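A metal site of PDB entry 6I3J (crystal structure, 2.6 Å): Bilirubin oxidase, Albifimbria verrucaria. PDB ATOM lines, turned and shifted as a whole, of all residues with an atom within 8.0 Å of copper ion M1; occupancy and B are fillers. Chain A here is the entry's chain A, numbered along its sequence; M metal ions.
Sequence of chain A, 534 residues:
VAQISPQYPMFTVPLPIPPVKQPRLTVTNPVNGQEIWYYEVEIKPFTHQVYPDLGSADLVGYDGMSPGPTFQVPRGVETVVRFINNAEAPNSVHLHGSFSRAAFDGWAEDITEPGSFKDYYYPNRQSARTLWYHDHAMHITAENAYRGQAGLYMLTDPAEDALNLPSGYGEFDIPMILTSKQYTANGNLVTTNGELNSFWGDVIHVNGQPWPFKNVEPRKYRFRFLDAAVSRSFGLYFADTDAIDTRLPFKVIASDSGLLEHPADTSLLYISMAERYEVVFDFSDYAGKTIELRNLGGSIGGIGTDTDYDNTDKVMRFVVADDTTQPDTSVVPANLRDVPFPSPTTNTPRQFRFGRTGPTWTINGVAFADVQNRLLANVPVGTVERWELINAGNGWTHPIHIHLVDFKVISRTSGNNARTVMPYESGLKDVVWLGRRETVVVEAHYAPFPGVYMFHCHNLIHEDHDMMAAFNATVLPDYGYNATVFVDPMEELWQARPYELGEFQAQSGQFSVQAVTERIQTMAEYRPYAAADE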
ATOM      1  N   HIS A  94      27.459 -23.614  13.705  1.00  0.00           N
ATOM      2  CA  HIS A  94      26.068 -23.605  14.049  1.00  0.00           C
ATOM      3  C   HIS A  94      25.666 -22.227  14.555  1.00  0.00           C
ATOM      4  O   HIS A  94      26.175 -21.781  15.599  1.00  0.00           O
ATOM      5  CB  HIS A  94      25.797 -24.635  15.144  1.00  0.00           C
ATOM      6  CG  HIS A  94      24.403 -24.555  15.658  1.00  0.00           C
ATOM      7  ND1 HIS A  94      23.313 -24.478  14.816  1.00  0.00           N
ATOM      8  CD2 HIS A  94      23.925 -24.497  16.923  1.00  0.00           C
ATOM      9  CE1 HIS A  94      22.225 -24.408  15.528  1.00  0.00           C
ATOM     10  NE2 HIS A  94      22.564 -24.432  16.817  1.00  0.00           N
ATOM     11  N   LEU A  95      24.729 -21.584  13.847  1.00  0.00           N
ATOM     12  CA  LEU A  95      24.037 -20.409  14.394  1.00  0.00           C
ATOM     13  C   LEU A  95      22.900 -20.856  15.331  1.00  0.00           C
ATOM     14  O   LEU A  95      21.803 -21.236  14.869  1.00  0.00           O
ATOM     15  CB  LEU A  95      23.494 -19.564  13.239  1.00  0.00           C
ATOM     16  CG  LEU A  95      22.833 -18.269  13.671  1.00  0.00           C
ATOM     17  CD1 LEU A  95      23.853 -17.361  14.333  1.00  0.00           C
ATOM     18  CD2 LEU A  95      22.177 -17.594  12.481  1.00  0.00           C
ATOM     19  N   HIS A  96      23.181 -20.801  16.648  1.00  0.00           N
ATOM     20  CA  HIS A  96      22.321 -21.311  17.736  1.00  0.00           C
ATOM     21  C   HIS A  96      21.155 -20.338  17.948  1.00  0.00           C
ATOM     22  O   HIS A  96      21.342 -19.147  18.251  1.00  0.00           O
ATOM     23  CB  HIS A  96      23.157 -21.514  19.005  1.00  0.00           C
ATOM     24  CG  HIS A  96      22.452 -22.198  20.136  1.00  0.00           C
ATOM     25  ND1 HIS A  96      22.994 -23.302  20.770  1.00  0.00           N
ATOM     26  CD2 HIS A  96      21.287 -21.931  20.771  1.00  0.00           C
ATOM     27  CE1 HIS A  96      22.180 -23.695  21.735  1.00  0.00           C
ATOM     28  NE2 HIS A  96      21.121 -22.870  21.749  1.00  0.00           N
ATOM     29  N   GLY A  97      19.939 -20.869  17.765  1.00  0.00           N
ATOM     30  CA  GLY A  97      18.706 -20.094  17.914  1.00  0.00           C
ATOM     31  C   GLY A  97      18.149 -19.590  16.592  1.00  0.00           C
ATOM     32  O   GLY A  97      17.256 -18.720  16.593  1.00  0.00           O
ATOM     33  N   TRP A 132      23.928 -17.019  19.053  1.00  0.00           N
ATOM     34  CA  TRP A 132      25.369 -17.077  19.070  1.00  0.00           C
ATOM     35  C   TRP A 132      25.773 -18.109  18.025  1.00  0.00           C
ATOM     36  O   TRP A 132      24.952 -18.961  17.701  1.00  0.00           O
ATOM     37  CB  TRP A 132      25.943 -17.344  20.486  1.00  0.00           C
ATOM     38  CG  TRP A 132      25.601 -18.666  21.124  1.00  0.00           C
ATOM     39  CD1 TRP A 132      24.361 -19.196  21.311  1.00  0.00           C
ATOM     40  CD2 TRP A 132      26.527 -19.608  21.705  1.00  0.00           C
ATOM     41  NE1 TRP A 132      24.439 -20.409  21.943  1.00  0.00           N
ATOM     42  CE2 TRP A 132      25.758 -20.685  22.204  1.00  0.00           C
ATOM     43  CE3 TRP A 132      27.919 -19.659  21.840  1.00  0.00           C
ATOM     44  CZ2 TRP A 132      26.341 -21.779  22.837  1.00  0.00           C
ATOM     45  CZ3 TRP A 132      28.493 -20.745  22.452  1.00  0.00           C
ATOM     46  CH2 TRP A 132      27.714 -21.783  22.957  1.00  0.00           C
ATOM     47  N   TYR A 133      26.963 -17.925  17.447  1.00  0.00           N
ATOM     48  CA  TYR A 133      27.496 -18.796  16.396  1.00  0.00           C
ATOM     49  C   TYR A 133      28.744 -19.444  16.992  1.00  0.00           C
ATOM     50  O   TYR A 133      29.522 -18.767  17.656  1.00  0.00           O
ATOM     51  CB  TYR A 133      27.722 -18.038  15.080  1.00  0.00           C
ATOM     52  CG  TYR A 133      28.785 -16.958  15.123  1.00  0.00           C
ATOM     53  CD1 TYR A 133      28.552 -15.726  15.701  1.00  0.00           C
ATOM     54  CD2 TYR A 133      30.045 -17.161  14.569  1.00  0.00           C
ATOM     55  CE1 TYR A 133      29.521 -14.742  15.758  1.00  0.00           C
ATOM     56  CE2 TYR A 133      31.024 -16.180  14.596  1.00  0.00           C
ATOM     57  CZ  TYR A 133      30.759 -14.967  15.196  1.00  0.00           C
ATOM     58  OH  TYR A 133      31.724 -14.006  15.227  1.00  0.00           O
ATOM     59  N   HIS A 134      28.863 -20.749  16.824  1.00  0.00           N
ATOM     60  CA  HIS A 134      29.945 -21.477  17.457  1.00  0.00           C
ATOM     61  C   HIS A 134      30.158 -22.794  16.733  1.00  0.00           C
ATOM     62  O   HIS A 134      29.303 -23.225  15.951  1.00  0.00           O
ATOM     63  CB  HIS A 134      29.664 -21.716  18.954  1.00  0.00           C
ATOM     64  CG  HIS A 134      28.517 -22.637  19.210  1.00  0.00           C
ATOM     65  ND1 HIS A 134      28.598 -24.003  19.002  1.00  0.00           N
ATOM     66  CD2 HIS A 134      27.266 -22.396  19.669  1.00  0.00           C
ATOM     67  CE1 HIS A 134      27.440 -24.560  19.311  1.00  0.00           C
ATOM     68  NE2 HIS A 134      26.610 -23.590  19.728  1.00  0.00           N
ATOM     69  N   ASP A 135      31.309 -23.410  17.007  1.00  0.00           N
ATOM     70  CA  ASP A 135      31.712 -24.610  16.342  1.00  0.00           C
ATOM     71  C   ASP A 135      30.882 -25.800  16.847  1.00  0.00           C
ATOM     72  O   ASP A 135      30.414 -25.816  18.005  1.00  0.00           O
ATOM     73  CB  ASP A 135      33.199 -24.880  16.530  1.00  0.00           C
ATOM     74  CG  ASP A 135      33.686 -25.946  15.576  1.00  0.00           C
ATOM     75  OD1 ASP A 135      33.560 -25.701  14.329  1.00  0.00           O
ATOM     76  OD2 ASP A 135      34.124 -27.023  16.083  1.00  0.00           O
ATOM     77  N   HIS A 136      30.723 -26.784  15.960  1.00  0.00           N
ATOM     78  CA  HIS A 136      29.857 -27.910  16.235  1.00  0.00           C
ATOM     79  C   HIS A 136      30.393 -29.188  15.566  1.00  0.00           C
ATOM     80  O   HIS A 136      29.635 -30.160  15.394  1.00  0.00           O
ATOM     81  CB  HIS A 136      28.446 -27.587  15.728  1.00  0.00           C
ATOM     82  CG  HIS A 136      27.353 -28.105  16.596  1.00  0.00           C
ATOM     83  ND1 HIS A 136      27.228 -29.445  16.907  1.00  0.00           N
ATOM     84  CD2 HIS A 136      26.326 -27.465  17.189  1.00  0.00           C
ATOM     85  CE1 HIS A 136      26.187 -29.594  17.674  1.00  0.00           C
ATOM     86  NE2 HIS A 136      25.614 -28.407  17.861  1.00  0.00           N
ATOM     87  N   THR A 141      34.161 -30.459  19.262  1.00  0.00           N
ATOM     88  CA  THR A 141      33.373 -29.244  19.510  1.00  0.00           C
ATOM     89  C   THR A 141      33.912 -28.531  20.750  1.00  0.00           C
ATOM     90  O   THR A 141      34.044 -27.306  20.780  1.00  0.00           O
ATOM     91  CB  THR A 141      31.869 -29.575  19.628  1.00  0.00           C
ATOM     92  OG1 THR A 141      31.352 -29.859  18.325  1.00  0.00           O
ATOM     93  CG2 THR A 141      31.060 -28.444  20.217  1.00  0.00           C
ATOM     94  N   LEU A 226      25.418 -14.932  28.010  1.00  0.00           N
ATOM     95  CA  LEU A 226      25.599 -16.187  27.293  1.00  0.00           C
ATOM     96  C   LEU A 226      26.536 -17.059  28.119  1.00  0.00           C
ATOM     97  O   LEU A 226      27.607 -16.597  28.531  1.00  0.00           O
ATOM     98  CB  LEU A 226      26.185 -15.923  25.897  1.00  0.00           C
ATOM     99  CG  LEU A 226      26.690 -17.148  25.120  1.00  0.00           C
ATOM    100  CD1 LEU A 226      25.634 -18.236  24.984  1.00  0.00           C
ATOM    101  CD2 LEU A 226      27.159 -16.731  23.746  1.00  0.00           C
ATOM    102  N   ASP A 227      26.120 -18.299  28.387  1.00  0.00           N
ATOM    103  CA  ASP A 227      27.045 -19.295  28.946  1.00  0.00           C
ATOM    104  C   ASP A 227      27.704 -20.030  27.781  1.00  0.00           C
ATOM    105  O   ASP A 227      27.119 -20.978  27.198  1.00  0.00           O
ATOM    106  CB  ASP A 227      26.370 -20.243  29.945  1.00  0.00           C
ATOM    107  CG  ASP A 227      27.340 -21.125  30.712  1.00  0.00           C
ATOM    108  OD1 ASP A 227      28.543 -21.110  30.381  1.00  0.00           O
ATOM    109  OD2 ASP A 227      26.887 -21.813  31.649  1.00  0.00           O
ATOM    110  N   MET A 273      25.068 -24.104  30.048  1.00  0.00           N
ATOM    111  CA  MET A 273      25.776 -24.025  28.749  1.00  0.00           C
ATOM    112  C   MET A 273      24.776 -23.799  27.611  1.00  0.00           C
ATOM    113  O   MET A 273      23.828 -24.585  27.413  1.00  0.00           O
ATOM    114  CB  MET A 273      26.594 -25.291  28.486  1.00  0.00           C
ATOM    115  CG  MET A 273      27.834 -25.418  29.376  1.00  0.00           C
ATOM    116  SD  MET A 273      27.537 -25.889  31.133  1.00  0.00           S
ATOM    117  CE  MET A 273      27.094 -27.618  30.973  1.00  0.00           C
ATOM    118  N   ALA A 274      24.975 -22.671  26.918  1.00  0.00           N
ATOM    119  CA  ALA A 274      24.313 -22.321  25.670  1.00  0.00           C
ATOM    120  C   ALA A 274      23.027 -21.540  25.914  1.00  0.00           C
ATOM    121  O   ALA A 274      22.381 -21.092  24.969  1.00  0.00           O
ATOM    122  CB  ALA A 274      24.042 -23.539  24.817  1.00  0.00           C
ATOM    123  N   GLU A 275      22.659 -21.357  27.182  1.00  0.00           N
ATOM    124  CA  GLU A 275      21.522 -20.497  27.532  1.00  0.00           C
ATOM    125  C   GLU A 275      21.900 -19.013  27.338  1.00  0.00           C
ATOM    126  O   GLU A 275      23.020 -18.592  27.647  1.00  0.00           O
ATOM    127  CB  GLU A 275      21.048 -20.774  28.965  1.00  0.00           C
ATOM    128  CG  GLU A 275      20.208 -22.037  29.060  1.00  0.00           C
ATOM    129  CD  GLU A 275      19.539 -22.281  30.393  1.00  0.00           C
ATOM    130  OE1 GLU A 275      20.201 -22.141  31.433  1.00  0.00           O
ATOM    131  OE2 GLU A 275      18.351 -22.634  30.367  1.00  0.00           O
ATOM    132  N   ARG A 276      20.949 -18.248  26.789  1.00  0.00           N
ATOM    133  CA  ARG A 276      21.022 -16.772  26.747  1.00  0.00           C
ATOM    134  C   ARG A 276      19.895 -16.220  27.646  1.00  0.00           C
ATOM    135  O   ARG A 276      18.723 -16.695  27.575  1.00  0.00           O
ATOM    136  CB  ARG A 276      20.954 -16.235  25.312  1.00  0.00           C
ATOM    137  CG  ARG A 276      22.098 -16.674  24.398  1.00  0.00           C
ATOM    138  CD  ARG A 276      21.892 -18.038  23.734  1.00  0.00           C
ATOM    139  NE  ARG A 276      20.775 -18.076  22.780  1.00  0.00           N
ATOM    140  CZ  ARG A 276      20.076 -19.170  22.448  1.00  0.00           C
ATOM    141  NH1 ARG A 276      19.230 -19.138  21.432  1.00  0.00           N
ATOM    142  NH2 ARG A 276      20.237 -20.300  23.133  1.00  0.00           N
ATOM    143  N   HIS A 401      19.666 -29.053  24.358  1.00  0.00           N
ATOM    144  CA  HIS A 401      19.398 -28.141  23.297  1.00  0.00           C
ATOM    145  C   HIS A 401      18.719 -28.918  22.173  1.00  0.00           C
ATOM    146  O   HIS A 401      19.170 -29.992  21.812  1.00  0.00           O
ATOM    147  CB  HIS A 401      20.716 -27.486  22.860  1.00  0.00           C
ATOM    148  CG  HIS A 401      20.551 -26.650  21.647  1.00  0.00           C
ATOM    149  ND1 HIS A 401      19.477 -25.790  21.489  1.00  0.00           N
ATOM    150  CD2 HIS A 401      21.309 -26.542  20.529  1.00  0.00           C
ATOM    151  CE1 HIS A 401      19.568 -25.178  20.336  1.00  0.00           C
ATOM    152  NE2 HIS A 401      20.696 -25.615  19.721  1.00  0.00           N
ATOM    153  N   HIS A 403      17.698 -28.339  18.244  1.00  0.00           N
ATOM    154  CA  HIS A 403      17.829 -27.487  17.055  1.00  0.00           C
ATOM    155  C   HIS A 403      16.452 -27.288  16.404  1.00  0.00           C
ATOM    156  O   HIS A 403      15.502 -28.007  16.707  1.00  0.00           O
ATOM    157  CB  HIS A 403      18.799 -28.098  16.043  1.00  0.00           C
ATOM    158  CG  HIS A 403      20.240 -28.067  16.473  1.00  0.00           C
ATOM    159  ND1 HIS A 403      21.210 -27.410  15.716  1.00  0.00           N
ATOM    160  CD2 HIS A 403      20.870 -28.615  17.529  1.00  0.00           C
ATOM    161  CE1 HIS A 403      22.378 -27.555  16.319  1.00  0.00           C
ATOM    162  NE2 HIS A 403      22.197 -28.312  17.436  1.00  0.00           N
ATOM    163  N   ASP A 430      15.410 -22.598  23.792  1.00  0.00           N
ATOM    164  CA  ASP A 430      15.961 -23.628  22.918  1.00  0.00           C
ATOM    165  C   ASP A 430      16.974 -24.476  23.680  1.00  0.00           C
ATOM    166  O   ASP A 430      17.508 -25.399  23.085  1.00  0.00           O
ATOM    167  CB  ASP A 430      16.539 -23.048  21.608  1.00  0.00           C
ATOM    168  CG  ASP A 430      17.650 -22.012  21.763  1.00  0.00           C
ATOM    169  OD1 ASP A 430      18.443 -22.156  22.715  1.00  0.00           O
ATOM    170  OD2 ASP A 430      17.723 -21.069  20.905  1.00  0.00           O
ATOM    171  N   VAL A 431      17.217 -24.163  24.960  1.00  0.00           N
ATOM    172  CA  VAL A 431      18.034 -24.976  25.901  1.00  0.00           C
ATOM    173  C   VAL A 431      17.333 -25.036  27.267  1.00  0.00           C
ATOM    174  O   VAL A 431      16.730 -24.075  27.712  1.00  0.00           O
ATOM    175  CB  VAL A 431      19.450 -24.392  26.059  1.00  0.00           C
ATOM    176  CG1 VAL A 431      20.349 -25.347  26.839  1.00  0.00           C
ATOM    177  CG2 VAL A 431      20.086 -24.051  24.719  1.00  0.00           C
ATOM    178  N   HIS A 456      20.835 -32.582  21.736  1.00  0.00           N
ATOM    179  CA  HIS A 456      21.937 -33.028  22.493  1.00  0.00           C
ATOM    180  C   HIS A 456      22.093 -32.239  23.775  1.00  0.00           C
ATOM    181  O   HIS A 456      21.527 -31.170  23.938  1.00  0.00           O
ATOM    182  CB  HIS A 456      23.219 -32.863  21.699  1.00  0.00           C
ATOM    183  CG  HIS A 456      23.503 -31.460  21.285  1.00  0.00           C
ATOM    184  ND1 HIS A 456      24.466 -30.692  21.908  1.00  0.00           N
ATOM    185  CD2 HIS A 456      22.996 -30.705  20.284  1.00  0.00           C
ATOM    186  CE1 HIS A 456      24.561 -29.537  21.295  1.00  0.00           C
ATOM    187  NE2 HIS A 456      23.676 -29.526  20.289  1.00  0.00           N
ATOM    188  N   HIS A 458      24.463 -29.890  25.933  1.00  0.00           N
ATOM    189  CA  HIS A 458      25.337 -28.789  25.510  1.00  0.00           C
ATOM    190  C   HIS A 458      26.521 -28.635  26.469  1.00  0.00           C
ATOM    191  O   HIS A 458      27.306 -27.674  26.364  1.00  0.00           O
ATOM    192  CB  HIS A 458      24.527 -27.489  25.315  1.00  0.00           C
ATOM    193  CG  HIS A 458      25.003 -26.650  24.154  1.00  0.00           C
ATOM    194  ND1 HIS A 458      26.246 -26.013  24.136  1.00  0.00           N
ATOM    195  CD2 HIS A 458      24.385 -26.344  22.987  1.00  0.00           C
ATOM    196  CE1 HIS A 458      26.367 -25.354  22.998  1.00  0.00           C
ATOM    197  NE2 HIS A 458      25.236 -25.539  22.270  1.00  0.00           N
ATOM    198  N   LEU A 460      29.833 -29.550  26.425  1.00  0.00           N
ATOM    199  CA  LEU A 460      30.586 -29.853  25.189  1.00  0.00           C
ATOM    200  C   LEU A 460      31.398 -31.158  25.342  1.00  0.00           C
ATOM    201  O   LEU A 460      31.598 -31.898  24.384  1.00  0.00           O
ATOM    202  CB  LEU A 460      31.465 -28.643  24.842  1.00  0.00           C
ATOM    203  CG  LEU A 460      30.718 -27.356  24.448  1.00  0.00           C
ATOM    204  CD1 LEU A 460      31.669 -26.346  23.791  1.00  0.00           C
ATOM    205  CD2 LEU A 460      29.546 -27.642  23.515  1.00  0.00           C
ATOM    206  N   GLU A 463      28.811 -33.792  24.984  1.00  0.00           N
ATOM    207  CA  GLU A 463      28.354 -33.683  23.597  1.00  0.00           C
ATOM    208  C   GLU A 463      29.325 -34.439  22.670  1.00  0.00           C
ATOM    209  O   GLU A 463      28.885 -35.135  21.741  1.00  0.00           O
ATOM    210  CB  GLU A 463      28.256 -32.202  23.215  1.00  0.00           C
ATOM    211  CG  GLU A 463      27.761 -31.881  21.793  1.00  0.00           C
ATOM    212  CD  GLU A 463      27.690 -30.399  21.436  1.00  0.00           C
ATOM    213  OE1 GLU A 463      27.396 -29.533  22.342  1.00  0.00           O
ATOM    214  OE2 GLU A 463      27.938 -30.074  20.231  1.00  0.00           O
HETATM  215 CU    CU M   1      24.910 -24.098  20.687  1.00  0.00          CU
HETATM  216 CU    CU M   2      21.427 -24.909  18.215  1.00  0.00          CU
HETATM  217 CU    CU M   3      23.792 -28.381  18.557  1.00  0.00          CU
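O of Trp 132 sits at hydrogen-bond distance from N of His 96 (2.8 Å). A ring nitrogen (NE2) of His 96 sits close to a ring nitrogen (ND1) of His 401 (3.4 Å). NE2 of His 96 is in hydrogen-bond range of NH2 of Arg 276 (3.0 Å). NE2 of His 94 sits close to ND1 of His 403 (3.5 Å). A ring nitrogen (NE2) of His 96 sits at hydrogen-bond distance from the side-chain carboxylate (OD1) of Asp 430 (2.9 Å). The backbone carbonyl oxygen (O) of His 134 lies within hydrogen-bond range of the backbone NH (N) of His 94 (2.9 Å).
Copper ion M1 is bound by a ring nitrogen (NE2) of His 134 (2.0 Å), a ring nitrogen (ND1) of His 96 (2.1 Å) and a ring nitrogen (NE2) of His 458 (2.2 Å). Copper ion M1 has three donor atoms within binding distance.
His 94 touches copper ion M1 (CD2 to CU, 3.9 Å). Trp 132 touches copper ion M1 (CZ2 to CU, 3.5 Å). Five residues have an atom within 4 Å of copper ion M1: His 94, His 96, Trp 132, His 134 and His 458. The nearest printed residue that does not touch copper ion M1 is Ala 274 (4.3 Å).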
